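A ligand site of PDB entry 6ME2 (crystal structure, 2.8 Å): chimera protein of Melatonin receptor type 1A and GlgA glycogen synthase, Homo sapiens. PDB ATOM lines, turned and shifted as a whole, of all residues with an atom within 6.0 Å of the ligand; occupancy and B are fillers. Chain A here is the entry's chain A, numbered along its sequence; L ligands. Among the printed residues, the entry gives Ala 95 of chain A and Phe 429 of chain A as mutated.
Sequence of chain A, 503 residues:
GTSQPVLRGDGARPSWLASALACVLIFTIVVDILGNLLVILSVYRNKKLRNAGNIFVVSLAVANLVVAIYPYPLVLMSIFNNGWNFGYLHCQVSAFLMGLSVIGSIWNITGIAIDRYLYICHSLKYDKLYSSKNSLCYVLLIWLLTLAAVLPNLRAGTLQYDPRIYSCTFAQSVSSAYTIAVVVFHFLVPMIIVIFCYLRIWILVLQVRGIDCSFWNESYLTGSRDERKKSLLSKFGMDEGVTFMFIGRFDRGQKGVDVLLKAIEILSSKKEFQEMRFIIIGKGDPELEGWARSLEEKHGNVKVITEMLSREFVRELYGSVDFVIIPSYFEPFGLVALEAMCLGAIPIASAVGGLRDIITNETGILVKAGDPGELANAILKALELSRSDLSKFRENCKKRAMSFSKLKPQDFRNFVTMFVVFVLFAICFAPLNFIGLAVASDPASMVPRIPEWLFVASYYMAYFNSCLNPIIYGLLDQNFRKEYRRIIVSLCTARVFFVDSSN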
ATOM      1  N   ALA A  95      18.485  20.678 -13.781  1.00  0.00           N
ATOM      2  CA  ALA A  95      17.025  20.701 -13.596  1.00  0.00           C
ATOM      3  C   ALA A  95      16.436  19.305 -13.789  1.00  0.00           C
ATOM      4  O   ALA A  95      15.599  18.891 -12.990  1.00  0.00           O
ATOM      5  CB  ALA A  95      16.395  21.684 -14.574  1.00  0.00           C
ATOM      6  N   PHE A  96      16.911  18.544 -14.815  1.00  0.00           N
ATOM      7  CA  PHE A  96      16.468  17.186 -15.128  1.00  0.00           C
ATOM      8  C   PHE A  96      16.766  16.202 -13.992  1.00  0.00           C
ATOM      9  O   PHE A  96      15.909  15.382 -13.675  1.00  0.00           O
ATOM     10  CB  PHE A  96      17.083  16.697 -16.460  1.00  0.00           C
ATOM     11  CG  PHE A  96      16.623  15.320 -16.905  1.00  0.00           C
ATOM     12  CD1 PHE A  96      15.417  15.165 -17.571  1.00  0.00           C
ATOM     13  CD2 PHE A  96      17.419  14.202 -16.683  1.00  0.00           C
ATOM     14  CE1 PHE A  96      14.991  13.894 -17.985  1.00  0.00           C
ATOM     15  CE2 PHE A  96      16.995  12.938 -17.102  1.00  0.00           C
ATOM     16  CZ  PHE A  96      15.786  12.797 -17.751  1.00  0.00           C
ATOM     17  N   MET A  98      17.167  16.981 -10.839  1.00  0.00           N
ATOM     18  CA  MET A  98      16.366  17.419  -9.690  1.00  0.00           C
ATOM     19  C   MET A  98      14.971  16.801  -9.780  1.00  0.00           C
ATOM     20  O   MET A  98      14.362  16.499  -8.754  1.00  0.00           O
ATOM     21  CB  MET A  98      16.272  18.945  -9.624  1.00  0.00           C
ATOM     22  CG  MET A  98      17.061  19.527  -8.493  1.00  0.00           C
ATOM     23  SD  MET A  98      16.821  21.307  -8.309  1.00  0.00           S
ATOM     24  CE  MET A  98      18.167  21.692  -7.219  1.00  0.00           C
ATOM     25  N   GLY A  99      14.499  16.624 -11.010  1.00  0.00           N
ATOM     26  CA  GLY A  99      13.217  15.995 -11.314  1.00  0.00           C
ATOM     27  C   GLY A  99      13.256  14.525 -10.966  1.00  0.00           C
ATOM     28  O   GLY A  99      12.416  14.055 -10.192  1.00  0.00           O
ATOM     29  N   LEU A 100      14.263  13.798 -11.495  1.00  0.00           N
ATOM     30  CA  LEU A 100      14.483  12.363 -11.243  1.00  0.00           C
ATOM     31  C   LEU A 100      14.550  12.057  -9.740  1.00  0.00           C
ATOM     32  O   LEU A 100      13.983  11.062  -9.285  1.00  0.00           O
ATOM     33  CB  LEU A 100      15.759  11.847 -11.927  1.00  0.00           C
ATOM     34  CG  LEU A 100      15.845  11.822 -13.464  1.00  0.00           C
ATOM     35  CD1 LEU A 100      17.192  11.275 -13.893  1.00  0.00           C
ATOM     36  CD2 LEU A 100      14.752  10.962 -14.081  1.00  0.00           C
ATOM     37  N   VAL A 102      13.376  14.136  -6.983  1.00  0.00           N
ATOM     38  CA  VAL A 102      12.107  14.477  -6.326  1.00  0.00           C
ATOM     39  C   VAL A 102      10.978  13.497  -6.689  1.00  0.00           C
ATOM     40  O   VAL A 102      10.289  13.032  -5.789  1.00  0.00           O
ATOM     41  CB  VAL A 102      11.729  15.969  -6.554  1.00  0.00           C
ATOM     42  CG1 VAL A 102      10.275  16.251  -6.175  1.00  0.00           C
ATOM     43  CG2 VAL A 102      12.666  16.897  -5.781  1.00  0.00           C
ATOM     44  N   ILE A 103      10.806  13.175  -7.995  1.00  0.00           N
ATOM     45  CA  ILE A 103       9.753  12.245  -8.470  1.00  0.00           C
ATOM     46  C   ILE A 103      10.041  10.810  -7.992  1.00  0.00           C
ATOM     47  O   ILE A 103       9.131  10.132  -7.520  1.00  0.00           O
ATOM     48  CB  ILE A 103       9.488  12.353 -10.017  1.00  0.00           C
ATOM     49  CG1 ILE A 103       9.151  13.819 -10.470  1.00  0.00           C
ATOM     50  CG2 ILE A 103       8.428  11.351 -10.505  1.00  0.00           C
ATOM     51  CD1 ILE A 103       7.958  14.573  -9.747  1.00  0.00           C
ATOM     52  N   ALA A 149       8.161  10.735 -16.717  1.00  0.00           N
ATOM     53  CA  ALA A 149       7.561  11.957 -16.205  1.00  0.00           C
ATOM     54  C   ALA A 149       8.439  13.203 -16.355  1.00  0.00           C
ATOM     55  O   ALA A 149       7.910  14.278 -16.630  1.00  0.00           O
ATOM     56  CB  ALA A 149       7.181  11.772 -14.742  1.00  0.00           C
ATOM     57  N   VAL A 150       9.755  13.067 -16.159  1.00  0.00           N
ATOM     58  CA  VAL A 150      10.719  14.178 -16.205  1.00  0.00           C
ATOM     59  C   VAL A 150      11.234  14.460 -17.646  1.00  0.00           C
ATOM     60  O   VAL A 150      11.519  15.618 -17.944  1.00  0.00           O
ATOM     61  CB  VAL A 150      11.883  13.985 -15.184  1.00  0.00           C
ATOM     62  CG1 VAL A 150      12.743  15.241 -15.070  1.00  0.00           C
ATOM     63  CG2 VAL A 150      11.344  13.607 -13.810  1.00  0.00           C
ATOM     64  N   ASN A 153       9.707  17.446 -20.083  1.00  0.00           N
ATOM     65  CA  ASN A 153      10.090  18.791 -19.637  1.00  0.00           C
ATOM     66  C   ASN A 153      11.281  19.388 -20.395  1.00  0.00           C
ATOM     67  O   ASN A 153      11.398  20.617 -20.484  1.00  0.00           O
ATOM     68  CB  ASN A 153      10.320  18.811 -18.135  1.00  0.00           C
ATOM     69  CG  ASN A 153       9.098  18.385 -17.363  1.00  0.00           C
ATOM     70  OD1 ASN A 153       8.122  19.124 -17.218  1.00  0.00           O
ATOM     71  ND2 ASN A 153       9.088  17.148 -16.909  1.00  0.00           N
ATOM     72  N   THR A 158      10.090  23.793 -20.156  1.00  0.00           N
ATOM     73  CA  THR A 158       9.515  24.206 -18.878  1.00  0.00           C
ATOM     74  C   THR A 158      10.606  24.223 -17.788  1.00  0.00           C
ATOM     75  O   THR A 158      10.318  24.495 -16.620  1.00  0.00           O
ATOM     76  CB  THR A 158       8.255  23.378 -18.572  1.00  0.00           C
ATOM     77  OG1 THR A 158       7.475  23.980 -17.537  1.00  0.00           O
ATOM     78  CG2 THR A 158       8.555  21.954 -18.244  1.00  0.00           C
ATOM     79  N   LEU A 159      11.874  23.972 -18.189  1.00  0.00           N
ATOM     80  CA  LEU A 159      13.022  23.988 -17.285  1.00  0.00           C
ATOM     81  C   LEU A 159      13.828  25.236 -17.558  1.00  0.00           C
ATOM     82  O   LEU A 159      14.345  25.410 -18.666  1.00  0.00           O
ATOM     83  CB  LEU A 159      13.914  22.742 -17.457  1.00  0.00           C
ATOM     84  CG  LEU A 159      13.282  21.370 -17.222  1.00  0.00           C
ATOM     85  CD1 LEU A 159      14.249  20.264 -17.590  1.00  0.00           C
ATOM     86  CD2 LEU A 159      12.823  21.212 -15.783  1.00  0.00           C
ATOM     87  N   THR A 169      15.233  24.938 -12.321  1.00  0.00           N
ATOM     88  CA  THR A 169      14.200  23.980 -11.907  1.00  0.00           C
ATOM     89  C   THR A 169      12.984  24.006 -12.862  1.00  0.00           C
ATOM     90  O   THR A 169      13.022  24.667 -13.908  1.00  0.00           O
ATOM     91  CB  THR A 169      13.834  24.263 -10.426  1.00  0.00           C
ATOM     92  OG1 THR A 169      12.993  23.228  -9.913  1.00  0.00           O
ATOM     93  CG2 THR A 169      13.187  25.629 -10.215  1.00  0.00           C
ATOM     94  N   PHE A 170      11.914  23.284 -12.486  1.00  0.00           N
ATOM     95  CA  PHE A 170      10.654  23.246 -13.219  1.00  0.00           C
ATOM     96  C   PHE A 170       9.920  24.563 -12.967  1.00  0.00           C
ATOM     97  O   PHE A 170       9.621  24.903 -11.814  1.00  0.00           O
ATOM     98  CB  PHE A 170       9.805  22.040 -12.768  1.00  0.00           C
ATOM     99  CG  PHE A 170       8.394  21.977 -13.312  1.00  0.00           C
ATOM    100  CD1 PHE A 170       8.130  21.371 -14.535  1.00  0.00           C
ATOM    101  CD2 PHE A 170       7.323  22.475 -12.584  1.00  0.00           C
ATOM    102  CE1 PHE A 170       6.827  21.289 -15.034  1.00  0.00           C
ATOM    103  CE2 PHE A 170       6.013  22.401 -13.073  1.00  0.00           C
ATOM    104  CZ  PHE A 170       5.773  21.801 -14.297  1.00  0.00           C
ATOM    105  N   GLN A 172       6.792  26.598 -12.837  1.00  0.00           N
ATOM    106  CA  GLN A 172       5.354  26.390 -12.649  1.00  0.00           C
ATOM    107  C   GLN A 172       4.528  27.316 -13.513  1.00  0.00           C
ATOM    108  O   GLN A 172       3.362  27.010 -13.771  1.00  0.00           O
ATOM    109  CB  GLN A 172       4.991  26.565 -11.175  1.00  0.00           C
ATOM    110  CG  GLN A 172       5.676  25.575 -10.239  1.00  0.00           C
ATOM    111  CD  GLN A 172       5.513  25.919  -8.779  1.00  0.00           C
ATOM    112  OE1 GLN A 172       5.334  27.081  -8.394  1.00  0.00           O
ATOM    113  NE2 GLN A 172       5.596  24.913  -7.933  1.00  0.00           N
ATOM    114  N   THR A 179       2.085  21.882 -14.926  1.00  0.00           N
ATOM    115  CA  THR A 179       2.104  22.173 -13.491  1.00  0.00           C
ATOM    116  C   THR A 179       1.011  21.407 -12.738  1.00  0.00           C
ATOM    117  O   THR A 179       1.306  20.760 -11.732  1.00  0.00           O
ATOM    118  CB  THR A 179       2.067  23.695 -13.258  1.00  0.00           C
ATOM    119  OG1 THR A 179       3.133  24.303 -14.010  1.00  0.00           O
ATOM    120  CG2 THR A 179       2.208  24.072 -11.787  1.00  0.00           C
ATOM    121  N   ILE A 180      -0.243  21.461 -13.244  1.00  0.00           N
ATOM    122  CA  ILE A 180      -1.425  20.768 -12.680  1.00  0.00           C
ATOM    123  C   ILE A 180      -1.196  19.253 -12.668  1.00  0.00           C
ATOM    124  O   ILE A 180      -1.395  18.627 -11.631  1.00  0.00           O
ATOM    125  CB  ILE A 180      -2.734  21.200 -13.397  1.00  0.00           C
ATOM    126  CG1 ILE A 180      -3.071  22.679 -13.118  1.00  0.00           C
ATOM    127  CG2 ILE A 180      -3.922  20.299 -13.010  1.00  0.00           C
ATOM    128  CD1 ILE A 180      -3.868  23.400 -14.212  1.00  0.00           C
ATOM    129  N   VAL A 182       1.665  17.594 -12.709  1.00  0.00           N
ATOM    130  CA  VAL A 182       2.726  17.288 -11.737  1.00  0.00           C
ATOM    131  C   VAL A 182       2.132  17.207 -10.308  1.00  0.00           C
ATOM    132  O   VAL A 182       2.387  16.234  -9.615  1.00  0.00           O
ATOM    133  CB  VAL A 182       3.948  18.254 -11.855  1.00  0.00           C
ATOM    134  CG1 VAL A 182       4.874  18.178 -10.639  1.00  0.00           C
ATOM    135  CG2 VAL A 182       4.744  17.968 -13.126  1.00  0.00           C
ATOM    136  N   VAL A 183       1.282  18.189  -9.931  1.00  0.00           N
ATOM    137  CA  VAL A 183       0.599  18.241  -8.628  1.00  0.00           C
ATOM    138  C   VAL A 183      -0.349  17.039  -8.478  1.00  0.00           C
ATOM    139  O   VAL A 183      -0.259  16.314  -7.491  1.00  0.00           O
ATOM    140  CB  VAL A 183      -0.160  19.587  -8.397  1.00  0.00           C
ATOM    141  CG1 VAL A 183      -0.973  19.553  -7.099  1.00  0.00           C
ATOM    142  CG2 VAL A 183       0.797  20.777  -8.391  1.00  0.00           C
ATOM    143  N   PHE A 429       7.163  19.159   1.053  1.00  0.00           N
ATOM    144  CA  PHE A 429       6.696  19.431  -0.307  1.00  0.00           C
ATOM    145  C   PHE A 429       5.268  19.992  -0.433  1.00  0.00           C
ATOM    146  O   PHE A 429       4.928  20.463  -1.520  1.00  0.00           O
ATOM    147  CB  PHE A 429       6.860  18.169  -1.173  1.00  0.00           C
ATOM    148  CG  PHE A 429       8.285  17.999  -1.651  1.00  0.00           C
ATOM    149  CD1 PHE A 429       9.231  17.336  -0.854  1.00  0.00           C
ATOM    150  CD2 PHE A 429       8.699  18.524  -2.870  1.00  0.00           C
ATOM    151  CE1 PHE A 429      10.543  17.197  -1.295  1.00  0.00           C
ATOM    152  CE2 PHE A 429      10.019  18.373  -3.306  1.00  0.00           C
ATOM    153  CZ  PHE A 429      10.931  17.708  -2.507  1.00  0.00           C
ATOM    154  N   LEU A 432       5.112  23.809  -1.703  1.00  0.00           N
ATOM    155  CA  LEU A 432       5.558  23.880  -3.093  1.00  0.00           C
ATOM    156  C   LEU A 432       4.430  23.513  -4.067  1.00  0.00           C
ATOM    157  O   LEU A 432       4.261  24.201  -5.061  1.00  0.00           O
ATOM    158  CB  LEU A 432       6.770  22.969  -3.320  1.00  0.00           C
ATOM    159  CG  LEU A 432       7.739  23.403  -4.423  1.00  0.00           C
ATOM    160  CD1 LEU A 432       8.646  24.521  -3.950  1.00  0.00           C
ATOM    161  CD2 LEU A 432       8.579  22.234  -4.901  1.00  0.00           C
ATOM    162  N   ASN A 433       3.675  22.446  -3.755  1.00  0.00           N
ATOM    163  CA  ASN A 433       2.555  22.007  -4.585  1.00  0.00           C
ATOM    164  C   ASN A 433       1.341  22.938  -4.483  1.00  0.00           C
ATOM    165  O   ASN A 433       0.594  23.074  -5.456  1.00  0.00           O
ATOM    166  CB  ASN A 433       2.201  20.546  -4.289  1.00  0.00           C
ATOM    167  CG  ASN A 433       3.241  19.581  -4.802  1.00  0.00           C
ATOM    168  OD1 ASN A 433       3.129  19.041  -5.902  1.00  0.00           O
ATOM    169  ND2 ASN A 433       4.298  19.378  -4.034  1.00  0.00           N
ATOM    170  N   GLY A 436       2.270  25.824  -6.545  1.00  0.00           N
ATOM    171  CA  GLY A 436       2.131  25.290  -7.902  1.00  0.00           C
ATOM    172  C   GLY A 436       0.732  25.471  -8.458  1.00  0.00           C
ATOM    173  O   GLY A 436       0.571  25.967  -9.569  1.00  0.00           O
ATOM    174  N   LEU A 437      -0.296  25.115  -7.645  1.00  0.00           N
ATOM    175  CA  LEU A 437      -1.714  25.247  -8.000  1.00  0.00           C
ATOM    176  C   LEU A 437      -2.122  26.724  -8.105  1.00  0.00           C
ATOM    177  O   LEU A 437      -2.902  27.081  -8.982  1.00  0.00           O
ATOM    178  CB  LEU A 437      -2.611  24.545  -6.977  1.00  0.00           C
ATOM    179  CG  LEU A 437      -2.603  23.019  -6.970  1.00  0.00           C
ATOM    180  CD1 LEU A 437      -3.329  22.495  -5.753  1.00  0.00           C
ATOM    181  CD2 LEU A 437      -3.238  22.442  -8.228  1.00  0.00           C
ATOM    182  N   TYR A 459      10.985  26.249  -1.462  1.00  0.00           N
ATOM    183  CA  TYR A 459      11.981  25.559  -2.286  1.00  0.00           C
ATOM    184  C   TYR A 459      13.109  24.995  -1.450  1.00  0.00           C
ATOM    185  O   TYR A 459      13.535  23.860  -1.698  1.00  0.00           O
ATOM    186  CB  TYR A 459      12.503  26.457  -3.414  1.00  0.00           C
ATOM    187  CG  TYR A 459      11.920  26.122  -4.774  1.00  0.00           C
ATOM    188  CD1 TYR A 459      12.370  25.014  -5.489  1.00  0.00           C
ATOM    189  CD2 TYR A 459      10.922  26.921  -5.337  1.00  0.00           C
ATOM    190  CE1 TYR A 459      11.821  24.693  -6.734  1.00  0.00           C
ATOM    191  CE2 TYR A 459      10.361  26.596  -6.575  1.00  0.00           C
ATOM    192  CZ  TYR A 459      10.815  25.491  -7.268  1.00  0.00           C
ATOM    193  OH  TYR A 459      10.265  25.160  -8.493  1.00  0.00           O
HETATM  194  C1  LIG L   1       7.876  19.795  -8.893  1.00  0.00           C
HETATM  195  C2  LIG L   1       6.328  21.570  -7.963  1.00  0.00           C
HETATM  196  C3  LIG L   1       5.721  21.743  -9.368  1.00  0.00           C
HETATM  197  O1  LIG L   1       5.930  22.262  -7.037  1.00  0.00           O
HETATM  198  C4  LIG L   1       4.189  21.737  -9.298  1.00  0.00           C
HETATM  199  O2  LIG L   1       9.690  17.914 -14.166  1.00  0.00           O
HETATM  200  C5  LIG L   1      11.524  19.586  -8.704  1.00  0.00           C
HETATM  201  C6  LIG L   1      12.534  19.842  -9.809  1.00  0.00           C
HETATM  202  C7  LIG L   1      11.985  19.382 -11.002  1.00  0.00           C
HETATM  203  C8  LIG L   1      12.577  19.297 -12.260  1.00  0.00           C
HETATM  204  C9  LIG L   1      11.851  18.782 -13.347  1.00  0.00           C
HETATM  205  C10 LIG L   1      10.523  18.390 -13.196  1.00  0.00           C
HETATM  206  C11 LIG L   1       8.575  17.310 -13.459  1.00  0.00           C
HETATM  207  C12 LIG L   1       8.536  18.008 -12.114  1.00  0.00           C
HETATM  208  C13 LIG L   1       9.937  18.498 -11.955  1.00  0.00           C
HETATM  209  C14 LIG L   1      10.655  18.982 -10.845  1.00  0.00           C
HETATM  210  C15 LIG L   1      10.247  19.195  -9.403  1.00  0.00           C
HETATM  211  C16 LIG L   1       9.240  20.338  -9.307  1.00  0.00           C
HETATM  212  N1  LIG L   1       7.325  20.655  -7.827  1.00  0.00           N
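The backbone carbonyl oxygen (O) of Leu 432 lies close to an oxygen (O1) of the ligand (3.2 Å).
Residues that only touch the ligand: Ala 95, Met 98, Gly 99, Leu 159, Thr 169, Phe 170, Thr 179, Val 182, Val 183 and Asn 433.
Hydrophobic or aromatic side chains within 4 Å of the ligand: Met 98, Leu 159, Phe 170, Val 182, Val 183 and Leu 432.
An oxygen (O1) of the ligand sits at hydrogen-bond distance from the side-chain amide nitrogen of Gln 172, at 2.8 Å.
ND2 of Asn 153 sits at hydrogen-bond distance from O2 of the ligand (2.9 Å).
The side-chain amide nitrogen (NE2) of Gln 172 is in hydrogen-bond range of the backbone carbonyl oxygen (O) of Leu 432, 3.2 Å away.
The backbone carbonyl oxygen (O) of Gln 172 is in hydrogen-bond range of the side-chain hydroxyl (OG1) of Thr 179.
ND2 of Asn 153 sits at hydrogen-bond distance from O of Val 150 (3.1 Å).
O of Ala 149 sits at hydrogen-bond distance from ND2 of Asn 153 (3.1 Å).
The backbone NH of Thr 158 sits at hydrogen-bond distance from the backbone carbonyl oxygen of Asn 153 (3.5 Å).
O of Phe 170 lies within hydrogen-bond range of OH of Tyr 459, at 3.4 Å.
ND2 of Asn 433 is in hydrogen-bond range of O of Phe 429 (2.8 Å).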
